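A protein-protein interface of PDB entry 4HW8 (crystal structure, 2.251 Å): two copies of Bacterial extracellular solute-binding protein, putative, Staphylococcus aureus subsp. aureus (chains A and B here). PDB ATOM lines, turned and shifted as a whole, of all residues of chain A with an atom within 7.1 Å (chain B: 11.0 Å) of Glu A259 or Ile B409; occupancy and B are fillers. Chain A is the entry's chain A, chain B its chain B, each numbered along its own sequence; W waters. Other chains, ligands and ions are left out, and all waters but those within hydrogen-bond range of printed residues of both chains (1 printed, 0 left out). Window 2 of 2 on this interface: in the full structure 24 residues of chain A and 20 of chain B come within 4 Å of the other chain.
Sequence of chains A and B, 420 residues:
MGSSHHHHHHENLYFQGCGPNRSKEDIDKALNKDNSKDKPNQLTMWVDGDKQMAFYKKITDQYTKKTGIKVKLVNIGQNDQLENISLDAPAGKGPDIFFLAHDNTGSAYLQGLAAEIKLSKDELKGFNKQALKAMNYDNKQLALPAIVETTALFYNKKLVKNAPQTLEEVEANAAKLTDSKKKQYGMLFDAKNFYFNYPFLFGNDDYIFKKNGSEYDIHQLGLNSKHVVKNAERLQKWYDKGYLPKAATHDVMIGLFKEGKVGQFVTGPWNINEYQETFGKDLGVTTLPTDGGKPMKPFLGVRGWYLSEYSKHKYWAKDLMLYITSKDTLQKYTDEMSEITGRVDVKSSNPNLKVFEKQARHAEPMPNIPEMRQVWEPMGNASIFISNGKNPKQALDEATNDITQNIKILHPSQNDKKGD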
ATOM      1  N   ASN A 156       6.143 -13.825  39.915  1.00  0.00           N
ATOM      2  CA  ASN A 156       4.905 -13.780  39.154  1.00  0.00           C
ATOM      3  C   ASN A 156       3.806 -14.359  40.033  1.00  0.00           C
ATOM      4  O   ASN A 156       3.826 -15.530  40.328  1.00  0.00           O
ATOM      5  CB  ASN A 156       5.116 -14.592  37.881  1.00  0.00           C
ATOM      6  CG  ASN A 156       3.875 -14.757  37.062  1.00  0.00           C
ATOM      7  OD1 ASN A 156       2.787 -14.318  37.447  1.00  0.00           O
ATOM      8  ND2 ASN A 156       4.029 -15.408  35.897  1.00  0.00           N
ATOM      9  N   LYS A 182       8.270 -27.615  29.363  1.00  0.00           N
ATOM     10  CA  LYS A 182       7.306 -26.529  29.219  1.00  0.00           C
ATOM     11  C   LYS A 182       8.046 -25.221  29.373  1.00  0.00           C
ATOM     12  O   LYS A 182       7.427 -24.165  29.390  1.00  0.00           O
ATOM     13  CB  LYS A 182       6.199 -26.601  30.271  1.00  0.00           C
ATOM     14  CG  LYS A 182       5.375 -27.873  30.237  1.00  0.00           C
ATOM     15  CD  LYS A 182       4.062 -27.725  31.051  1.00  0.00           C
ATOM     16  CE  LYS A 182       4.292 -27.265  32.509  1.00  0.00           C
ATOM     17  NZ  LYS A 182       3.081 -27.418  33.387  1.00  0.00           N
ATOM     18  N   LYS A 183       9.373 -25.288  29.459  1.00  0.00           N
ATOM     19  CA  LYS A 183      10.204 -24.107  29.726  1.00  0.00           C
ATOM     20  C   LYS A 183       9.678 -23.346  30.954  1.00  0.00           C
ATOM     21  O   LYS A 183       9.728 -22.128  30.963  1.00  0.00           O
ATOM     22  CB  LYS A 183      10.302 -23.146  28.516  1.00  0.00           C
ATOM     23  CG  LYS A 183      11.077 -23.678  27.298  1.00  0.00           C
ATOM     24  CD  LYS A 183      10.940 -22.735  26.072  1.00  0.00           C
ATOM     25  CE  LYS A 183      11.514 -23.365  24.789  1.00  0.00           C
ATOM     26  NZ  LYS A 183      11.154 -22.585  23.555  1.00  0.00           N
ATOM     27  N   ALA A 248      20.516 -21.102  29.150  1.00  0.00           N
ATOM     28  CA  ALA A 248      19.973 -19.733  29.191  1.00  0.00           C
ATOM     29  C   ALA A 248      20.969 -18.661  29.639  1.00  0.00           C
ATOM     30  O   ALA A 248      21.752 -18.872  30.543  1.00  0.00           O
ATOM     31  CB  ALA A 248      18.715 -19.683  30.091  1.00  0.00           C
ATOM     32  N   ASP A 251      19.586 -12.561  29.251  1.00  0.00           N
ATOM     33  CA  ASP A 251      18.583 -12.060  28.321  1.00  0.00           C
ATOM     34  C   ASP A 251      17.502 -13.089  28.050  1.00  0.00           C
ATOM     35  O   ASP A 251      16.356 -12.700  27.867  1.00  0.00           O
ATOM     36  CB  ASP A 251      19.199 -11.543  27.007  1.00  0.00           C
ATOM     37  CG  ASP A 251      19.925 -10.198  27.179  1.00  0.00           C
ATOM     38  OD1 ASP A 251      19.667  -9.485  28.172  1.00  0.00           O
ATOM     39  OD2 ASP A 251      20.734  -9.846  26.310  1.00  0.00           O
ATOM     40  N   VAL A 252      17.850 -14.378  28.024  1.00  0.00           N
ATOM     41  CA  VAL A 252      16.846 -15.420  27.818  1.00  0.00           C
ATOM     42  C   VAL A 252      15.934 -15.497  29.051  1.00  0.00           C
ATOM     43  O   VAL A 252      14.710 -15.641  28.931  1.00  0.00           O
ATOM     44  CB  VAL A 252      17.489 -16.812  27.587  1.00  0.00           C
ATOM     45  CG1 VAL A 252      16.447 -17.902  27.641  1.00  0.00           C
ATOM     46  CG2 VAL A 252      18.233 -16.839  26.294  1.00  0.00           C
ATOM     47  N   MET A 253      16.546 -15.400  30.234  1.00  0.00           N
ATOM     48  CA  MET A 253      15.811 -15.454  31.479  1.00  0.00           C
ATOM     49  C   MET A 253      14.794 -14.345  31.549  1.00  0.00           C
ATOM     50  O   MET A 253      13.678 -14.548  32.010  1.00  0.00           O
ATOM     51  CB  MET A 253      16.760 -15.423  32.681  1.00  0.00           C
ATOM     52  CG  MET A 253      17.579 -16.710  32.777  1.00  0.00           C
ATOM     53  SD  MET A 253      18.658 -16.714  34.176  1.00  0.00           S
ATOM     54  CE  MET A 253      19.508 -18.307  34.006  1.00  0.00           C
ATOM     55  N   ILE A 254      15.170 -13.171  31.071  1.00  0.00           N
ATOM     56  CA  ILE A 254      14.262 -12.050  31.034  1.00  0.00           C
ATOM     57  C   ILE A 254      13.074 -12.414  30.163  1.00  0.00           C
ATOM     58  O   ILE A 254      11.940 -12.137  30.527  1.00  0.00           O
ATOM     59  CB  ILE A 254      14.937 -10.814  30.450  1.00  0.00           C
ATOM     60  CG1 ILE A 254      16.032 -10.317  31.406  1.00  0.00           C
ATOM     61  CG2 ILE A 254      13.918  -9.696  30.186  1.00  0.00           C
ATOM     62  CD1 ILE A 254      16.844  -9.133  30.818  1.00  0.00           C
ATOM     63  N   GLY A 255      13.351 -13.038  29.023  1.00  0.00           N
ATOM     64  CA  GLY A 255      12.308 -13.435  28.067  1.00  0.00           C
ATOM     65  C   GLY A 255      11.337 -14.441  28.678  1.00  0.00           C
ATOM     66  O   GLY A 255      10.129 -14.254  28.631  1.00  0.00           O
ATOM     67  N   LEU A 256      11.880 -15.499  29.263  1.00  0.00           N
ATOM     68  CA  LEU A 256      11.069 -16.518  29.916  1.00  0.00           C
ATOM     69  C   LEU A 256      10.189 -15.915  31.013  1.00  0.00           C
ATOM     70  O   LEU A 256       8.998 -16.216  31.080  1.00  0.00           O
ATOM     71  CB  LEU A 256      11.964 -17.630  30.469  1.00  0.00           C
ATOM     72  CG  LEU A 256      12.735 -18.408  29.397  1.00  0.00           C
ATOM     73  CD1 LEU A 256      13.644 -19.453  30.005  1.00  0.00           C
ATOM     74  CD2 LEU A 256      11.755 -19.029  28.420  1.00  0.00           C
ATOM     75  N   PHE A 257      10.754 -15.041  31.846  1.00  0.00           N
ATOM     76  CA  PHE A 257       9.967 -14.386  32.907  1.00  0.00           C
ATOM     77  C   PHE A 257       8.795 -13.600  32.332  1.00  0.00           C
ATOM     78  O   PHE A 257       7.663 -13.704  32.823  1.00  0.00           O
ATOM     79  CB  PHE A 257      10.838 -13.477  33.775  1.00  0.00           C
ATOM     80  CG  PHE A 257      10.096 -12.843  34.908  1.00  0.00           C
ATOM     81  CD1 PHE A 257       9.798 -13.569  36.045  1.00  0.00           C
ATOM     82  CD2 PHE A 257       9.706 -11.510  34.848  1.00  0.00           C
ATOM     83  CE1 PHE A 257       9.101 -12.994  37.110  1.00  0.00           C
ATOM     84  CE2 PHE A 257       9.003 -10.926  35.908  1.00  0.00           C
ATOM     85  CZ  PHE A 257       8.705 -11.675  37.035  1.00  0.00           C
ATOM     86  N   LYS A 258       9.059 -12.834  31.284  1.00  0.00           N
ATOM     87  CA  LYS A 258       8.005 -12.079  30.627  1.00  0.00           C
ATOM     88  C   LYS A 258       6.957 -12.957  29.949  1.00  0.00           C
ATOM     89  O   LYS A 258       5.823 -12.524  29.800  1.00  0.00           O
ATOM     90  CB  LYS A 258       8.559 -11.071  29.632  1.00  0.00           C
ATOM     91  CG  LYS A 258       9.321  -9.950  30.310  1.00  0.00           C
ATOM     92  CD  LYS A 258       9.302  -8.653  29.495  1.00  0.00           C
ATOM     93  CE  LYS A 258       9.975  -8.741  28.150  1.00  0.00           C
ATOM     94  NZ  LYS A 258       9.696  -7.443  27.398  1.00  0.00           N
ATOM     95  N   GLU A 259       7.328 -14.169  29.534  1.00  0.00           N
ATOM     96  CA  GLU A 259       6.359 -15.091  28.935  1.00  0.00           C
ATOM     97  C   GLU A 259       5.474 -15.758  29.994  1.00  0.00           C
ATOM     98  O   GLU A 259       4.576 -16.513  29.656  1.00  0.00           O
ATOM     99  CB  GLU A 259       7.041 -16.189  28.126  1.00  0.00           C
ATOM    100  CG  GLU A 259       7.655 -15.759  26.799  1.00  0.00           C
ATOM    101  CD  GLU A 259       8.247 -16.944  26.016  1.00  0.00           C
ATOM    102  OE1 GLU A 259       9.014 -16.708  25.044  1.00  0.00           O
ATOM    103  OE2 GLU A 259       7.942 -18.111  26.371  1.00  0.00           O
ATOM    104  N   GLY A 260       5.720 -15.498  31.270  1.00  0.00           N
ATOM    105  CA  GLY A 260       4.901 -16.093  32.326  1.00  0.00           C
ATOM    106  C   GLY A 260       5.309 -17.518  32.645  1.00  0.00           C
ATOM    107  O   GLY A 260       4.528 -18.285  33.190  1.00  0.00           O
ATOM    108  N   LYS A 261       6.553 -17.862  32.327  1.00  0.00           N
ATOM    109  CA  LYS A 261       7.055 -19.206  32.547  1.00  0.00           C
ATOM    110  C   LYS A 261       7.965 -19.365  33.759  1.00  0.00           C
ATOM    111  O   LYS A 261       8.481 -20.465  33.976  1.00  0.00           O
ATOM    112  CB  LYS A 261       7.793 -19.678  31.283  1.00  0.00           C
ATOM    113  CG  LYS A 261       6.857 -19.861  30.086  1.00  0.00           C
ATOM    114  CD  LYS A 261       7.423 -20.771  29.014  1.00  0.00           C
ATOM    115  CE  LYS A 261       6.310 -21.236  28.058  1.00  0.00           C
ATOM    116  NZ  LYS A 261       6.740 -22.346  27.146  1.00  0.00           N
ATOM    117  N   VAL A 262       8.112 -18.309  34.566  1.00  0.00           N
ATOM    118  CA  VAL A 262       9.068 -18.266  35.682  1.00  0.00           C
ATOM    119  C   VAL A 262       8.441 -17.678  36.947  1.00  0.00           C
ATOM    120  O   VAL A 262       7.943 -16.538  36.953  1.00  0.00           O
ATOM    121  CB  VAL A 262      10.322 -17.402  35.274  1.00  0.00           C
ATOM    122  CG1 VAL A 262      11.319 -17.206  36.450  1.00  0.00           C
ATOM    123  CG2 VAL A 262      11.025 -18.036  34.050  1.00  0.00           C
ATOM    124  N   THR A 278       3.612  -5.737  31.567  1.00  0.00           N
ATOM    125  CA  THR A 278       3.242  -7.110  31.260  1.00  0.00           C
ATOM    126  C   THR A 278       2.340  -7.733  32.303  1.00  0.00           C
ATOM    127  O   THR A 278       1.290  -8.245  31.970  1.00  0.00           O
ATOM    128  CB  THR A 278       4.490  -8.003  31.130  1.00  0.00           C
ATOM    129  OG1 THR A 278       5.298  -7.509  30.068  1.00  0.00           O
ATOM    130  CG2 THR A 278       4.122  -9.475  30.856  1.00  0.00           C
ATOM    131  N   PHE A 279       2.726  -7.656  33.568  1.00  0.00           N
ATOM    132  CA  PHE A 279       1.974  -8.325  34.635  1.00  0.00           C
ATOM    133  C   PHE A 279       0.995  -7.508  35.470  1.00  0.00           C
ATOM    134  O   PHE A 279       0.110  -8.084  36.073  1.00  0.00           O
ATOM    135  CB  PHE A 279       2.950  -9.005  35.582  1.00  0.00           C
ATOM    136  CG  PHE A 279       3.727 -10.107  34.941  1.00  0.00           C
ATOM    137  CD1 PHE A 279       3.077 -11.262  34.521  1.00  0.00           C
ATOM    138  CD2 PHE A 279       5.092 -10.004  34.766  1.00  0.00           C
ATOM    139  CE1 PHE A 279       3.774 -12.283  33.923  1.00  0.00           C
ATOM    140  CE2 PHE A 279       5.804 -11.031  34.178  1.00  0.00           C
ATOM    141  CZ  PHE A 279       5.147 -12.175  33.761  1.00  0.00           C
ATOM    142  N   ILE B 218      19.087 -17.338   9.871  1.00  0.00           N
ATOM    143  CA  ILE B 218      19.235 -17.526  11.322  1.00  0.00           C
ATOM    144  C   ILE B 218      19.026 -18.966  11.782  1.00  0.00           C
ATOM    145  O   ILE B 218      19.319 -19.300  12.933  1.00  0.00           O
ATOM    146  CB  ILE B 218      18.286 -16.598  12.139  1.00  0.00           C
ATOM    147  CG1 ILE B 218      16.815 -16.977  11.929  1.00  0.00           C
ATOM    148  CG2 ILE B 218      18.542 -15.128  11.789  1.00  0.00           C
ATOM    149  CD1 ILE B 218      15.833 -16.205  12.799  1.00  0.00           C
ATOM    150  N   HIS B 219      18.509 -19.809  10.889  1.00  0.00           N
ATOM    151  CA  HIS B 219      18.278 -21.220  11.193  1.00  0.00           C
ATOM    152  C   HIS B 219      19.355 -22.158  10.630  1.00  0.00           C
ATOM    153  O   HIS B 219      19.201 -23.367  10.682  1.00  0.00           O
ATOM    154  CB  HIS B 219      16.922 -21.636  10.667  1.00  0.00           C
ATOM    155  CG  HIS B 219      15.792 -20.879  11.281  1.00  0.00           C
ATOM    156  ND1 HIS B 219      15.028 -19.979  10.571  1.00  0.00           N
ATOM    157  CD2 HIS B 219      15.312 -20.869  12.545  1.00  0.00           C
ATOM    158  CE1 HIS B 219      14.109 -19.464  11.367  1.00  0.00           C
ATOM    159  NE2 HIS B 219      14.261 -19.986  12.570  1.00  0.00           N
ATOM    160  N   PRO B 370      19.958  -9.078  14.790  1.00  0.00           N
ATOM    161  CA  PRO B 370      19.678  -9.193  16.217  1.00  0.00           C
ATOM    162  C   PRO B 370      20.027 -10.561  16.805  1.00  0.00           C
ATOM    163  O   PRO B 370      20.454 -10.649  17.953  1.00  0.00           O
ATOM    164  CB  PRO B 370      18.160  -8.941  16.306  1.00  0.00           C
ATOM    165  CG  PRO B 370      17.829  -8.181  15.069  1.00  0.00           C
ATOM    166  CD  PRO B 370      18.767  -8.665  14.023  1.00  0.00           C
ATOM    167  N   GLU B 371      19.859 -11.608  16.010  1.00  0.00           N
ATOM    168  CA  GLU B 371      20.119 -12.962  16.466  1.00  0.00           C
ATOM    169  C   GLU B 371      21.600 -13.189  16.738  1.00  0.00           C
ATOM    170  O   GLU B 371      21.953 -14.139  17.439  1.00  0.00           O
ATOM    171  CB  GLU B 371      19.604 -13.999  15.466  1.00  0.00           C
ATOM    172  CG  GLU B 371      18.077 -14.019  15.248  1.00  0.00           C
ATOM    173  CD  GLU B 371      17.582 -12.873  14.369  1.00  0.00           C
ATOM    174  OE1 GLU B 371      18.426 -12.067  13.894  1.00  0.00           O
ATOM    175  OE2 GLU B 371      16.356 -12.787  14.145  1.00  0.00           O
ATOM    176  N   GLN B 374      22.708 -13.603  20.362  1.00  0.00           N
ATOM    177  CA  GLN B 374      22.582 -14.887  21.041  1.00  0.00           C
ATOM    178  C   GLN B 374      23.798 -15.781  20.880  1.00  0.00           C
ATOM    179  O   GLN B 374      23.969 -16.740  21.630  1.00  0.00           O
ATOM    180  CB  GLN B 374      21.320 -15.634  20.582  1.00  0.00           C
ATOM    181  CG  GLN B 374      20.049 -15.202  21.265  1.00  0.00           C
ATOM    182  CD  GLN B 374      19.668 -13.787  20.972  1.00  0.00           C
ATOM    183  OE1 GLN B 374      19.854 -12.881  21.805  1.00  0.00           O
ATOM    184  NE2 GLN B 374      19.158 -13.566  19.778  1.00  0.00           N
ATOM    185  N   PRO B 378      27.242 -18.247  24.363  1.00  0.00           N
ATOM    186  CA  PRO B 378      27.444 -19.673  24.202  1.00  0.00           C
ATOM    187  C   PRO B 378      28.796 -20.002  23.538  1.00  0.00           C
ATOM    188  O   PRO B 378      29.423 -20.984  23.913  1.00  0.00           O
ATOM    189  CB  PRO B 378      26.269 -20.098  23.323  1.00  0.00           C
ATOM    190  CG  PRO B 378      25.197 -19.140  23.673  1.00  0.00           C
ATOM    191  CD  PRO B 378      25.913 -17.824  23.893  1.00  0.00           C
ATOM    192  N   ASN B 401      23.443 -25.966  19.853  1.00  0.00           N
ATOM    193  CA  ASN B 401      22.142 -26.336  20.387  1.00  0.00           C
ATOM    194  C   ASN B 401      21.588 -25.187  21.225  1.00  0.00           C
ATOM    195  O   ASN B 401      20.447 -24.750  21.038  1.00  0.00           O
ATOM    196  CB  ASN B 401      22.266 -27.593  21.247  1.00  0.00           C
ATOM    197  CG  ASN B 401      20.948 -28.013  21.866  1.00  0.00           C
ATOM    198  OD1 ASN B 401      19.873 -27.593  21.429  1.00  0.00           O
ATOM    199  ND2 ASN B 401      21.022 -28.859  22.883  1.00  0.00           N
ATOM    200  N   ASP B 402      22.421 -24.689  22.132  1.00  0.00           N
ATOM    201  CA  ASP B 402      22.032 -23.576  23.018  1.00  0.00           C
ATOM    202  C   ASP B 402      21.654 -22.294  22.236  1.00  0.00           C
ATOM    203  O   ASP B 402      20.635 -21.650  22.519  1.00  0.00           O
ATOM    204  CB  ASP B 402      23.124 -23.291  24.031  1.00  0.00           C
ATOM    205  CG  ASP B 402      23.331 -24.452  25.025  1.00  0.00           C
ATOM    206  OD1 ASP B 402      22.589 -25.450  24.968  1.00  0.00           O
ATOM    207  OD2 ASP B 402      24.254 -24.357  25.873  1.00  0.00           O
ATOM    208  N   ILE B 403      22.442 -21.959  21.224  1.00  0.00           N
ATOM    209  CA  ILE B 403      22.144 -20.784  20.394  1.00  0.00           C
ATOM    210  C   ILE B 403      20.810 -20.970  19.694  1.00  0.00           C
ATOM    211  O   ILE B 403      19.966 -20.071  19.678  1.00  0.00           O
ATOM    212  CB  ILE B 403      23.255 -20.537  19.362  1.00  0.00           C
ATOM    213  CG1 ILE B 403      24.517 -20.067  20.077  1.00  0.00           C
ATOM    214  CG2 ILE B 403      22.817 -19.509  18.349  1.00  0.00           C
ATOM    215  CD1 ILE B 403      25.771 -20.171  19.218  1.00  0.00           C
ATOM    216  N   THR B 404      20.613 -22.149  19.124  1.00  0.00           N
ATOM    217  CA  THR B 404      19.355 -22.458  18.435  1.00  0.00           C
ATOM    218  C   THR B 404      18.151 -22.246  19.345  1.00  0.00           C
ATOM    219  O   THR B 404      17.230 -21.534  18.969  1.00  0.00           O
ATOM    220  CB  THR B 404      19.314 -23.897  17.920  1.00  0.00           C
ATOM    221  OG1 THR B 404      20.426 -24.120  17.039  1.00  0.00           O
ATOM    222  CG2 THR B 404      17.971 -24.170  17.181  1.00  0.00           C
ATOM    223  N   GLN B 405      18.167 -22.839  20.541  1.00  0.00           N
ATOM    224  CA  GLN B 405      17.024 -22.713  21.434  1.00  0.00           C
ATOM    225  C   GLN B 405      16.865 -21.291  22.001  1.00  0.00           C
ATOM    226  O   GLN B 405      15.749 -20.845  22.248  1.00  0.00           O
ATOM    227  CB  GLN B 405      17.054 -23.766  22.554  1.00  0.00           C
ATOM    228  CG  GLN B 405      17.771 -23.386  23.829  1.00  0.00           C
ATOM    229  CD  GLN B 405      17.808 -24.559  24.827  1.00  0.00           C
ATOM    230  OE1 GLN B 405      17.134 -24.537  25.864  1.00  0.00           O
ATOM    231  NE2 GLN B 405      18.568 -25.605  24.483  1.00  0.00           N
ATOM    232  N   ASN B 406      17.970 -20.573  22.189  1.00  0.00           N
ATOM    233  CA  ASN B 406      17.881 -19.205  22.704  1.00  0.00           C
ATOM    234  C   ASN B 406      17.303 -18.250  21.663  1.00  0.00           C
ATOM    235  O   ASN B 406      16.538 -17.339  22.011  1.00  0.00           O
ATOM    236  CB  ASN B 406      19.231 -18.715  23.243  1.00  0.00           C
ATOM    237  CG  ASN B 406      19.637 -19.438  24.507  1.00  0.00           C
ATOM    238  OD1 ASN B 406      18.826 -20.115  25.100  1.00  0.00           O
ATOM    239  ND2 ASN B 406      20.893 -19.286  24.927  1.00  0.00           N
ATOM    240  N   ILE B 407      17.651 -18.462  20.391  1.00  0.00           N
ATOM    241  CA  ILE B 407      17.100 -17.642  19.318  1.00  0.00           C
ATOM    242  C   ILE B 407      15.599 -17.853  19.277  1.00  0.00           C
ATOM    243  O   ILE B 407      14.845 -16.881  19.228  1.00  0.00           O
ATOM    244  CB  ILE B 407      17.765 -17.920  17.958  1.00  0.00           C
ATOM    245  CG1 ILE B 407      19.159 -17.277  17.910  1.00  0.00           C
ATOM    246  CG2 ILE B 407      16.918 -17.360  16.809  1.00  0.00           C
ATOM    247  CD1 ILE B 407      19.928 -17.536  16.574  1.00  0.00           C
ATOM    248  N   LYS B 408      15.156 -19.109  19.358  1.00  0.00           N
ATOM    249  CA  LYS B 408      13.720 -19.408  19.345  1.00  0.00           C
ATOM    250  C   LYS B 408      12.981 -18.687  20.471  1.00  0.00           C
ATOM    251  O   LYS B 408      11.865 -18.207  20.275  1.00  0.00           O
ATOM    252  CB  LYS B 408      13.445 -20.914  19.483  1.00  0.00           C
ATOM    253  CG  LYS B 408      13.851 -21.741  18.283  1.00  0.00           C
ATOM    254  CD  LYS B 408      13.537 -23.256  18.447  1.00  0.00           C
ATOM    255  CE  LYS B 408      14.225 -24.069  17.317  1.00  0.00           C
ATOM    256  NZ  LYS B 408      14.246 -25.548  17.567  1.00  0.00           N
ATOM    257  N   ILE B 409      13.597 -18.637  21.650  1.00  0.00           N
ATOM    258  CA  ILE B 409      12.977 -18.008  22.816  1.00  0.00           C
ATOM    259  C   ILE B 409      12.864 -16.506  22.635  1.00  0.00           C
ATOM    260  O   ILE B 409      11.793 -15.937  22.802  1.00  0.00           O
ATOM    261  CB  ILE B 409      13.758 -18.323  24.118  1.00  0.00           C
ATOM    262  CG1 ILE B 409      13.578 -19.797  24.495  1.00  0.00           C
ATOM    263  CG2 ILE B 409      13.262 -17.455  25.278  1.00  0.00           C
ATOM    264  CD1 ILE B 409      14.532 -20.266  25.565  1.00  0.00           C
ATOM    265  N   LEU B 410      13.968 -15.870  22.266  1.00  0.00           N
ATOM    266  CA  LEU B 410      13.984 -14.423  22.102  1.00  0.00           C
ATOM    267  C   LEU B 410      13.497 -13.928  20.733  1.00  0.00           C
ATOM    268  O   LEU B 410      13.247 -12.733  20.573  1.00  0.00           O
ATOM    269  CB  LEU B 410      15.391 -13.888  22.403  1.00  0.00           C
ATOM    270  CG  LEU B 410      15.807 -14.095  23.862  1.00  0.00           C
ATOM    271  CD1 LEU B 410      17.189 -13.500  24.120  1.00  0.00           C
ATOM    272  CD2 LEU B 410      14.758 -13.456  24.755  1.00  0.00           C
ATOM    273  N   HIS B 411      13.380 -14.825  19.749  1.00  0.00           N
ATOM    274  CA  HIS B 411      12.909 -14.438  18.403  1.00  0.00           C
ATOM    275  C   HIS B 411      12.039 -15.521  17.795  1.00  0.00           C
ATOM    276  O   HIS B 411      12.449 -16.197  16.849  1.00  0.00           O
ATOM    277  CB  HIS B 411      14.075 -14.167  17.455  1.00  0.00           C
ATOM    278  CG  HIS B 411      15.043 -13.157  17.967  1.00  0.00           C
ATOM    279  ND1 HIS B 411      14.821 -11.800  17.879  1.00  0.00           N
ATOM    280  CD2 HIS B 411      16.244 -13.307  18.570  1.00  0.00           C
ATOM    281  CE1 HIS B 411      15.841 -11.159  18.417  1.00  0.00           C
ATOM    282  NE2 HIS B 411      16.722 -12.052  18.833  1.00  0.00           N
ATOM    283  N   PRO B 412      10.825 -15.680  18.313  1.00  0.00           N
ATOM    284  CA  PRO B 412       9.928 -16.713  17.774  1.00  0.00           C
ATOM    285  C   PRO B 412       9.804 -16.690  16.234  1.00  0.00           C
ATOM    286  O   PRO B 412       8.814 -16.203  15.679  1.00  0.00           O
ATOM    287  CB  PRO B 412       8.606 -16.401  18.461  1.00  0.00           C
ATOM    288  CG  PRO B 412       9.019 -15.808  19.777  1.00  0.00           C
ATOM    289  CD  PRO B 412      10.241 -14.990  19.479  1.00  0.00           C
HETATM  290  O   HOH W   1      13.789 -22.680  22.633  1.00  0.00           O
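O of Leu A256 is in hydrogen-bond range of N of Lys A261 (3.2 Å). O of Asp B402 lies close to ND2 of Asn B406, at 3.4 Å.
CG1 of Ile B409 touches NZ of Lys A183, 3.8 Å away. Leu B410 touches Asp A251 (CD2 to O, 3.6 Å). CG2 of Val A252 touches CG of Asn B406, 3.5 Å away. Val A252 touches Ile B409 (CG1 to CD1, 3.7 Å). Leu A256 touches Ile B409 (CD2 to CG2, 3.8 Å). Ile B409 touches Glu A259 (O to OE1, 3.7 Å).
Lys A182 touches none of the printed residues of chain B. Of the printed residues of chain B, Lys A183 touches Ile B409. Printed residues of chain B within 4 Å of Asp A251: Leu B410 (3.6 Å). No residue of chain B comes within 4 Å of Gly A255. Of the printed residues of chain B, Leu A256 touches Ile B409 (3.8 Å). Glu A259 touches just one residue of chain B: Ile B409. Ile B407 touches none of the printed residues of chain A. The nearest printed residue of chain B that does not touch Lys A183 is Lys B408 (5.0 Å).
Of the 18 printed residues of chain A, 5 touch a printed residue of chain B. Of the 18 printed residues of chain B, 3 touch a printed residue of chain A. Among the printed residues, no Asp or Glu carboxylate lies within 4 Å of a Lys or Arg side-chain nitrogen of the other chain.
No position is printed for both chains. Of the 6 pairs that touch across the chains among the printed residues, none has its exchanged pair printed and touching as well.
Water W1 lies within hydrogen-bond range of the backbone carbonyl oxygen of Gln B405 and the side-chain amino group of Lys A183.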
